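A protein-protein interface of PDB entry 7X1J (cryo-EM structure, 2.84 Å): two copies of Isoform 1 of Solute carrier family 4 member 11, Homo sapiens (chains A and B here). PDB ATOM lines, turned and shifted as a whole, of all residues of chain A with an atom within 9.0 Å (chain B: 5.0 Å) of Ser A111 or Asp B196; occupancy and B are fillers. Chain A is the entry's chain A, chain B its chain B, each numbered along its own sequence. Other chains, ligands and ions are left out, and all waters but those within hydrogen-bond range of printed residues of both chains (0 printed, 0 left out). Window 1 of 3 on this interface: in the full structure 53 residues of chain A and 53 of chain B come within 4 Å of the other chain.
The backbone carbonyl oxygen (O) of Ser B195 lies within hydrogen-bond range of the backbone NH (N) of Arg A112 (2.8 Å). OD1 of Asp B196 sits at hydrogen-bond distance from OG of Ser A111, 2.9 Å away. The backbone carbonyl oxygen of His A109 sits close to the backbone carbonyl oxygen of Ser B111 (3.2 Å). N of Thr B110 sits at hydrogen-bond distance from O of Thr A197 (3.1 Å). The backbone carbonyl oxygen (O) of Leu B194 sits at hydrogen-bond distance from the guanidinium group (NH1) of Arg A112. The guanidinium group (NH1) of Arg B112 lies within hydrogen-bond range of the backbone carbonyl oxygen (O) of Leu A194, at 3.2 Å. NE2 of His A109 lies close to SD of Met B266 (3.4 Å). The backbone carbonyl oxygen (O) of Lys A113 is in hydrogen-bond range of the backbone NH (N) of His B109 (2.7 Å). N of Ser B111 lies within hydrogen-bond range of O of Ser A111 (2.7 Å). O of Thr B197 sits at hydrogen-bond distance from N of Thr A110 (3.1 Å). The backbone NH (N) of Arg B112 lies within hydrogen-bond range of the backbone carbonyl oxygen (O) of Ser A195, 2.8 Å away. The backbone carbonyl oxygen of Ser A111 sits close to the backbone carbonyl oxygen of His B109, 3.2 Å away. The side-chain carboxylate (OD1) of Asp A196 is in hydrogen-bond range of the side-chain hydroxyl (OG) of Ser B111 (2.9 Å).
OG of Ser A111 lies within hydrogen-bond range of NZ of Lys A113. The backbone carbonyl oxygen (O) of Cys B216 sits at hydrogen-bond distance from the backbone NH (N) of Ile B198, at 3.0 Å. N of Ile B218 lies within hydrogen-bond range of O of Asp B196 (3.1 Å).
Among the printed residues, pairs that only touch across the chains: Ser A111 with Thr B110, Thr A110 with Ser B111, His A109 with Arg B112, Arg A112 with His B109, Ser A111 with Ser B195, Ser A195 with Ser B111, His A109 with Thr B197, Thr A197 with His B109, Leu A108 with Ile B198, Thr A110 with Thr B110, Asp A196 with Thr B110, Thr A110 with Asp B196, Thr A197 with Arg B112, Arg A112 with Thr B197, Leu A108 with Thr B197, Ser A195 with Thr B110, Thr A110 with Ser B195, Thr A110 with Arg B112, Arg A112 with Thr B110, His A109 with Asp B196 and Asp A196 with His B109.
Of the printed residues of chain B, Leu A108 touches Thr B197 and Ile B198. Ser A111 touches just these residues of chain B: His B109, Thr B110, Ser B111, Ser B195 and Asp B196. Tyr A114 touches none of the printed residues of chain B. Printed residues of chain B within 4 Å of Asp A196: His B109 (3.98 Å), Thr B110 (3.7 Å) and Ser B111 (2.9 Å). Printed residues of chain A within 4 Å of His B109: Ser A111 (3.2 Å), Arg A112 (3.2 Å), Lys A113 (2.7 Å), Asp A196 (3.98 Å) and Thr A197 (3.3 Å). Of the printed residues of chain A, Ser B111 touches His A109 (3.2 Å), Thr A110 (3.0 Å), Ser A111 (2.7 Å), Ser A195 (3.2 Å) and Asp A196 (2.9 Å). Ser B195 touches three residues of chain A. Printed residues of chain A within 4 Å of Asp B196: His A109 (3.98 Å), Thr A110 (3.7 Å) and Ser A111 (2.9 Å). Of chain A, only Leu A108, His A109, Thr A110 and Arg A112 come within 4 Å of Thr B197. Of the printed residues of chain A, Ile B198 touches Leu A108. No residue of chain A comes within 4 Å of Ile B218. The nearest residue of chain A that does not touch Asp B196 is Lys A113 (4.3 Å). The nearest printed residue of chain A that does not touch Ser B111 is Arg A112 (4.9 Å).
Hydrophobic or aromatic side chains of chain A that line the printed part of chain B: His A109. Hydrophobic or aromatic side chains of chain B within 4 Å of the printed part of chain A: His B109 and Met B266. Among the printed residues, no Asp or Glu carboxylate lies within 4 Å of a Lys or Arg side-chain nitrogen of the other chain.
His A109 touches Thr B197, and with the chains exchanged Thr A197 touches His B109. Thr A110 touches Ser B111, and with the chains exchanged Ser A111 touches Thr B110. Thr A110 touches Ser B195, and with the chains exchanged Ser A195 touches Thr B110. Arg A112 touches Leu B194, and with the chains exchanged Leu A194 touches Arg B112. Positions printed for both chains: 109, 110, 111, 112, 194, 195, 196 and 197. Of the 34 pairs that touch across the chains among the printed residues, 30 have their exchanged pair printed and touching as well.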
ATOM      1  N   LEU A 108       6.790   1.310  14.922  1.00  0.00           N
ATOM      2  CA  LEU A 108       6.961   0.750  13.588  1.00  0.00           C
ATOM      3  C   LEU A 108       5.589   0.427  13.006  1.00  0.00           C
ATOM      4  O   LEU A 108       4.836  -0.366  13.584  1.00  0.00           O
ATOM      5  CB  LEU A 108       7.843  -0.499  13.632  1.00  0.00           C
ATOM      6  CG  LEU A 108       8.153  -1.202  12.307  1.00  0.00           C
ATOM      7  CD1 LEU A 108       9.617  -1.610  12.256  1.00  0.00           C
ATOM      8  CD2 LEU A 108       7.258  -2.417  12.114  1.00  0.00           C
ATOM      9  N   HIS A 109       5.270   1.039  11.869  1.00  0.00           N
ATOM     10  CA  HIS A 109       4.001   0.823  11.181  1.00  0.00           C
ATOM     11  C   HIS A 109       4.245  -0.098   9.991  1.00  0.00           C
ATOM     12  O   HIS A 109       4.926   0.281   9.033  1.00  0.00           O
ATOM     13  CB  HIS A 109       3.395   2.150  10.730  1.00  0.00           C
ATOM     14  CG  HIS A 109       2.143   2.000   9.920  1.00  0.00           C
ATOM     15  ND1 HIS A 109       1.783   2.895   8.936  1.00  0.00           N
ATOM     16  CD2 HIS A 109       1.169   1.061   9.950  1.00  0.00           C
ATOM     17  CE1 HIS A 109       0.641   2.512   8.393  1.00  0.00           C
ATOM     18  NE2 HIS A 109       0.247   1.402   8.991  1.00  0.00           N
ATOM     19  N   THR A 110       3.692  -1.305  10.054  1.00  0.00           N
ATOM     20  CA  THR A 110       3.795  -2.282   8.979  1.00  0.00           C
ATOM     21  C   THR A 110       2.437  -2.441   8.308  1.00  0.00           C
ATOM     22  O   THR A 110       1.429  -2.673   8.984  1.00  0.00           O
ATOM     23  CB  THR A 110       4.296  -3.630   9.505  1.00  0.00           C
ATOM     24  OG1 THR A 110       3.956  -4.667   8.576  1.00  0.00           O
ATOM     25  CG2 THR A 110       3.688  -3.940  10.867  1.00  0.00           C
ATOM     26  N   SER A 111       2.414  -2.306   6.985  1.00  0.00           N
ATOM     27  CA  SER A 111       1.198  -2.440   6.193  1.00  0.00           C
ATOM     28  C   SER A 111       1.389  -3.545   5.167  1.00  0.00           C
ATOM     29  O   SER A 111       2.383  -3.550   4.432  1.00  0.00           O
ATOM     30  CB  SER A 111       0.843  -1.124   5.495  1.00  0.00           C
ATOM     31  OG  SER A 111      -0.344  -1.255   4.732  1.00  0.00           O
ATOM     32  N   ARG A 112       0.439  -4.475   5.118  1.00  0.00           N
ATOM     33  CA  ARG A 112       0.477  -5.600   4.194  1.00  0.00           C
ATOM     34  C   ARG A 112      -0.710  -5.507   3.246  1.00  0.00           C
ATOM     35  O   ARG A 112      -1.854  -5.372   3.692  1.00  0.00           O
ATOM     36  CB  ARG A 112       0.455  -6.931   4.949  1.00  0.00           C
ATOM     37  CG  ARG A 112       1.575  -7.083   5.966  1.00  0.00           C
ATOM     38  CD  ARG A 112       1.444  -8.380   6.746  1.00  0.00           C
ATOM     39  NE  ARG A 112       2.490  -8.518   7.753  1.00  0.00           N
ATOM     40  CZ  ARG A 112       2.402  -8.055   8.993  1.00  0.00           C
ATOM     41  NH1 ARG A 112       1.326  -7.414   9.418  1.00  0.00           N
ATOM     42  NH2 ARG A 112       3.422  -8.240   9.827  1.00  0.00           N
ATOM     43  N   LYS A 113      -0.434  -5.582   1.946  1.00  0.00           N
ATOM     44  CA  LYS A 113      -1.467  -5.496   0.923  1.00  0.00           C
ATOM     45  C   LYS A 113      -1.197  -6.537  -0.152  1.00  0.00           C
ATOM     46  O   LYS A 113      -0.044  -6.776  -0.518  1.00  0.00           O
ATOM     47  CB  LYS A 113      -1.523  -4.097   0.295  1.00  0.00           C
ATOM     48  CG  LYS A 113      -1.934  -2.992   1.256  1.00  0.00           C
ATOM     49  CD  LYS A 113      -1.947  -1.638   0.566  1.00  0.00           C
ATOM     50  CE  LYS A 113      -2.397  -0.538   1.515  1.00  0.00           C
ATOM     51  NZ  LYS A 113      -1.501  -0.427   2.698  1.00  0.00           N
ATOM     52  N   TYR A 114      -2.266  -7.151  -0.653  1.00  0.00           N
ATOM     53  CA  TYR A 114      -2.145  -8.132  -1.721  1.00  0.00           C
ATOM     54  C   TYR A 114      -1.999  -7.429  -3.063  1.00  0.00           C
ATOM     55  O   TYR A 114      -2.751  -6.500  -3.375  1.00  0.00           O
ATOM     56  CB  TYR A 114      -3.359  -9.061  -1.739  1.00  0.00           C
ATOM     57  CG  TYR A 114      -3.330 -10.135  -0.676  1.00  0.00           C
ATOM     58  CD1 TYR A 114      -2.170 -10.401   0.040  1.00  0.00           C
ATOM     59  CD2 TYR A 114      -4.460 -10.891  -0.394  1.00  0.00           C
ATOM     60  CE1 TYR A 114      -2.137 -11.384   1.010  1.00  0.00           C
ATOM     61  CE2 TYR A 114      -4.439 -11.877   0.573  1.00  0.00           C
ATOM     62  CZ  TYR A 114      -3.274 -12.120   1.272  1.00  0.00           C
ATOM     63  OH  TYR A 114      -3.249 -13.100   2.238  1.00  0.00           O
ATOM     64  N   LEU A 194      13.341  -4.510   6.927  1.00  0.00           N
ATOM     65  CA  LEU A 194      13.350  -3.940   5.588  1.00  0.00           C
ATOM     66  C   LEU A 194      12.138  -3.041   5.380  1.00  0.00           C
ATOM     67  O   LEU A 194      11.040  -3.328   5.865  1.00  0.00           O
ATOM     68  CB  LEU A 194      13.374  -5.051   4.538  1.00  0.00           C
ATOM     69  CG  LEU A 194      14.703  -5.799   4.395  1.00  0.00           C
ATOM     70  CD1 LEU A 194      14.534  -7.051   3.550  1.00  0.00           C
ATOM     71  CD2 LEU A 194      15.759  -4.887   3.791  1.00  0.00           C
ATOM     72  N   SER A 195      12.347  -1.940   4.655  1.00  0.00           N
ATOM     73  CA  SER A 195      11.279  -0.964   4.465  1.00  0.00           C
ATOM     74  C   SER A 195      10.176  -1.510   3.567  1.00  0.00           C
ATOM     75  O   SER A 195       8.988  -1.409   3.896  1.00  0.00           O
ATOM     76  CB  SER A 195      11.854   0.329   3.887  1.00  0.00           C
ATOM     77  OG  SER A 195      10.836   1.292   3.675  1.00  0.00           O
ATOM     78  N   ASP A 196      10.548  -2.101   2.432  1.00  0.00           N
ATOM     79  CA  ASP A 196       9.577  -2.589   1.462  1.00  0.00           C
ATOM     80  C   ASP A 196      10.001  -3.964   0.967  1.00  0.00           C
ATOM     81  O   ASP A 196      11.156  -4.156   0.578  1.00  0.00           O
ATOM     82  CB  ASP A 196       9.446  -1.624   0.278  1.00  0.00           C
ATOM     83  CG  ASP A 196       8.902  -0.269   0.687  1.00  0.00           C
ATOM     84  OD1 ASP A 196       7.968  -0.226   1.515  1.00  0.00           O
ATOM     85  OD2 ASP A 196       9.410   0.754   0.181  1.00  0.00           O
ATOM     86  N   THR A 197       9.060  -4.906   0.971  1.00  0.00           N
ATOM     87  CA  THR A 197       9.324  -6.264   0.516  1.00  0.00           C
ATOM     88  C   THR A 197       8.071  -6.824  -0.140  1.00  0.00           C
ATOM     89  O   THR A 197       6.948  -6.411   0.163  1.00  0.00           O
ATOM     90  CB  THR A 197       9.762  -7.181   1.667  1.00  0.00           C
ATOM     91  OG1 THR A 197       8.998  -6.881   2.843  1.00  0.00           O
ATOM     92  CG2 THR A 197      11.245  -7.015   1.964  1.00  0.00           C
ATOM     93  N   TYR A 210       3.058 -18.531   3.233  1.00  0.00           N
ATOM     94  CA  TYR A 210       4.072 -17.689   2.616  1.00  0.00           C
ATOM     95  C   TYR A 210       5.103 -18.534   1.880  1.00  0.00           C
ATOM     96  O   TYR A 210       5.354 -19.693   2.225  1.00  0.00           O
ATOM     97  CB  TYR A 210       4.766 -16.824   3.669  1.00  0.00           C
ATOM     98  CG  TYR A 210       3.938 -15.650   4.144  1.00  0.00           C
ATOM     99  CD1 TYR A 210       2.896 -15.831   5.045  1.00  0.00           C
ATOM    100  CD2 TYR A 210       4.205 -14.363   3.698  1.00  0.00           C
ATOM    101  CE1 TYR A 210       2.139 -14.760   5.483  1.00  0.00           C
ATOM    102  CE2 TYR A 210       3.455 -13.286   4.132  1.00  0.00           C
ATOM    103  CZ  TYR A 210       2.423 -13.491   5.023  1.00  0.00           C
ATOM    104  OH  TYR A 210       1.673 -12.422   5.458  1.00  0.00           O
ATOM    105  N   HIS B 109       2.570  -7.393  -0.304  1.00  0.00           N
ATOM    106  CA  HIS B 109       3.467  -6.248  -0.176  1.00  0.00           C
ATOM    107  C   HIS B 109       3.380  -5.720   1.250  1.00  0.00           C
ATOM    108  O   HIS B 109       2.339  -5.201   1.666  1.00  0.00           O
ATOM    109  CB  HIS B 109       3.104  -5.160  -1.184  1.00  0.00           C
ATOM    110  CG  HIS B 109       3.914  -3.907  -1.041  1.00  0.00           C
ATOM    111  ND1 HIS B 109       3.415  -2.661  -1.351  1.00  0.00           N
ATOM    112  CD2 HIS B 109       5.186  -3.710  -0.623  1.00  0.00           C
ATOM    113  CE1 HIS B 109       4.346  -1.750  -1.128  1.00  0.00           C
ATOM    114  NE2 HIS B 109       5.429  -2.360  -0.686  1.00  0.00           N
ATOM    115  N   THR B 110       4.472  -5.854   1.998  1.00  0.00           N
ATOM    116  CA  THR B 110       4.562  -5.360   3.365  1.00  0.00           C
ATOM    117  C   THR B 110       5.505  -4.165   3.409  1.00  0.00           C
ATOM    118  O   THR B 110       6.637  -4.242   2.921  1.00  0.00           O
ATOM    119  CB  THR B 110       5.042  -6.458   4.318  1.00  0.00           C
ATOM    120  OG1 THR B 110       5.560  -5.866   5.516  1.00  0.00           O
ATOM    121  CG2 THR B 110       6.117  -7.314   3.660  1.00  0.00           C
ATOM    122  N   SER B 111       5.030  -3.062   3.986  1.00  0.00           N
ATOM    123  CA  SER B 111       5.810  -1.838   4.118  1.00  0.00           C
ATOM    124  C   SER B 111       5.912  -1.469   5.589  1.00  0.00           C
ATOM    125  O   SER B 111       4.897  -1.411   6.292  1.00  0.00           O
ATOM    126  CB  SER B 111       5.176  -0.690   3.327  1.00  0.00           C
ATOM    127  OG  SER B 111       5.939   0.497   3.451  1.00  0.00           O
ATOM    128  N   ARG B 112       7.137  -1.219   6.050  1.00  0.00           N
ATOM    129  CA  ARG B 112       7.403  -0.857   7.434  1.00  0.00           C
ATOM    130  C   ARG B 112       7.990   0.545   7.478  1.00  0.00           C
ATOM    131  O   ARG B 112       8.964   0.837   6.775  1.00  0.00           O
ATOM    132  CB  ARG B 112       8.361  -1.857   8.088  1.00  0.00           C
ATOM    133  CG  ARG B 112       7.880  -3.298   8.034  1.00  0.00           C
ATOM    134  CD  ARG B 112       8.912  -4.250   8.613  1.00  0.00           C
ATOM    135  NE  ARG B 112       8.480  -5.641   8.529  1.00  0.00           N
ATOM    136  CZ  ARG B 112       8.699  -6.433   7.488  1.00  0.00           C
ATOM    137  NH1 ARG B 112       9.347  -6.005   6.418  1.00  0.00           N
ATOM    138  NH2 ARG B 112       8.256  -7.687   7.523  1.00  0.00           N
ATOM    139  N   LEU B 194      -2.454  -9.445   9.231  1.00  0.00           N
ATOM    140  CA  LEU B 194      -3.186  -8.212   9.481  1.00  0.00           C
ATOM    141  C   LEU B 194      -2.768  -7.131   8.492  1.00  0.00           C
ATOM    142  O   LEU B 194      -1.597  -7.027   8.118  1.00  0.00           O
ATOM    143  CB  LEU B 194      -2.955  -7.738  10.915  1.00  0.00           C
ATOM    144  CG  LEU B 194      -3.656  -8.556  12.005  1.00  0.00           C
ATOM    145  CD1 LEU B 194      -3.133  -8.186  13.383  1.00  0.00           C
ATOM    146  CD2 LEU B 194      -5.160  -8.349  11.932  1.00  0.00           C
ATOM    147  N   SER B 195      -3.742  -6.324   8.065  1.00  0.00           N
ATOM    148  CA  SER B 195      -3.472  -5.309   7.051  1.00  0.00           C
ATOM    149  C   SER B 195      -2.600  -4.188   7.602  1.00  0.00           C
ATOM    150  O   SER B 195      -1.610  -3.793   6.973  1.00  0.00           O
ATOM    151  CB  SER B 195      -4.790  -4.752   6.511  1.00  0.00           C
ATOM    152  OG  SER B 195      -4.559  -3.750   5.536  1.00  0.00           O
ATOM    153  N   ASP B 196      -2.943  -3.668   8.779  1.00  0.00           N
ATOM    154  CA  ASP B 196      -2.229  -2.541   9.363  1.00  0.00           C
ATOM    155  C   ASP B 196      -1.998  -2.799  10.845  1.00  0.00           C
ATOM    156  O   ASP B 196      -2.932  -3.158  11.567  1.00  0.00           O
ATOM    157  CB  ASP B 196      -3.009  -1.235   9.175  1.00  0.00           C
ATOM    158  CG  ASP B 196      -3.161  -0.852   7.716  1.00  0.00           C
ATOM    159  OD1 ASP B 196      -2.183  -1.003   6.954  1.00  0.00           O
ATOM    160  OD2 ASP B 196      -4.260  -0.400   7.331  1.00  0.00           O
ATOM    161  N   THR B 197      -0.759  -2.601  11.290  1.00  0.00           N
ATOM    162  CA  THR B 197      -0.398  -2.800  12.687  1.00  0.00           C
ATOM    163  C   THR B 197       0.676  -1.797  13.075  1.00  0.00           C
ATOM    164  O   THR B 197       1.442  -1.318  12.233  1.00  0.00           O
ATOM    165  CB  THR B 197       0.103  -4.227  12.953  1.00  0.00           C
ATOM    166  OG1 THR B 197       0.922  -4.664  11.859  1.00  0.00           O
ATOM    167  CG2 THR B 197      -1.060  -5.191  13.138  1.00  0.00           C
ATOM    168  N   ILE B 198       0.721  -1.483  14.368  1.00  0.00           N
ATOM    169  CA  ILE B 198       1.742  -0.615  14.941  1.00  0.00           C
ATOM    170  C   ILE B 198       2.356  -1.333  16.134  1.00  0.00           C
ATOM    171  O   ILE B 198       1.632  -1.816  17.013  1.00  0.00           O
ATOM    172  CB  ILE B 198       1.169   0.751  15.364  1.00  0.00           C
ATOM    173  CG1 ILE B 198       0.864   1.605  14.131  1.00  0.00           C
ATOM    174  CG2 ILE B 198       2.128   1.476  16.296  1.00  0.00           C
ATOM    175  CD1 ILE B 198       0.411   3.013  14.456  1.00  0.00           C
ATOM    176  N   CYS B 216      -1.136  -3.214  18.371  1.00  0.00           N
ATOM    177  CA  CYS B 216      -2.137  -2.228  17.973  1.00  0.00           C
ATOM    178  C   CYS B 216      -2.604  -2.558  16.562  1.00  0.00           C
ATOM    179  O   CYS B 216      -1.815  -2.503  15.613  1.00  0.00           O
ATOM    180  CB  CYS B 216      -1.570  -0.811  18.050  1.00  0.00           C
ATOM    181  SG  CYS B 216      -2.760   0.489  17.650  1.00  0.00           S
ATOM    182  N   ILE B 217      -3.883  -2.904  16.428  1.00  0.00           N
ATOM    183  CA  ILE B 217      -4.473  -3.285  15.150  1.00  0.00           C
ATOM    184  C   ILE B 217      -5.303  -2.125  14.624  1.00  0.00           C
ATOM    185  O   ILE B 217      -6.084  -1.514  15.365  1.00  0.00           O
ATOM    186  CB  ILE B 217      -5.323  -4.562  15.296  1.00  0.00           C
ATOM    187  CG1 ILE B 217      -4.482  -5.676  15.925  1.00  0.00           C
ATOM    188  CG2 ILE B 217      -5.871  -5.002  13.947  1.00  0.00           C
ATOM    189  CD1 ILE B 217      -5.238  -6.957  16.165  1.00  0.00           C
ATOM    190  N   ILE B 218      -5.135  -1.815  13.339  1.00  0.00           N
ATOM    191  CA  ILE B 218      -5.777  -0.668  12.709  1.00  0.00           C
ATOM    192  C   ILE B 218      -6.546  -1.149  11.487  1.00  0.00           C
ATOM    193  O   ILE B 218      -6.083  -2.034  10.758  1.00  0.00           O
ATOM    194  CB  ILE B 218      -4.755   0.414  12.302  1.00  0.00           C
ATOM    195  CG1 ILE B 218      -3.671   0.575  13.367  1.00  0.00           C
ATOM    196  CG2 ILE B 218      -5.453   1.742  12.068  1.00  0.00           C
ATOM    197  CD1 ILE B 218      -2.616   1.592  12.994  1.00  0.00           C
ATOM    198  N   MET B 266      -4.463   6.196  11.627  1.00  0.00           N
ATOM    199  CA  MET B 266      -3.074   6.144  12.075  1.00  0.00           C
ATOM    200  C   MET B 266      -2.841   7.069  13.263  1.00  0.00           C
ATOM    201  O   MET B 266      -2.168   6.697  14.232  1.00  0.00           O
ATOM    202  CB  MET B 266      -2.140   6.506  10.919  1.00  0.00           C
ATOM    203  CG  MET B 266      -2.236   5.560   9.737  1.00  0.00           C
ATOM    204  SD  MET B 266      -1.700   3.895  10.167  1.00  0.00           S
ATOM    205  CE  MET B 266      -2.945   2.915   9.333  1.00  0.00           C
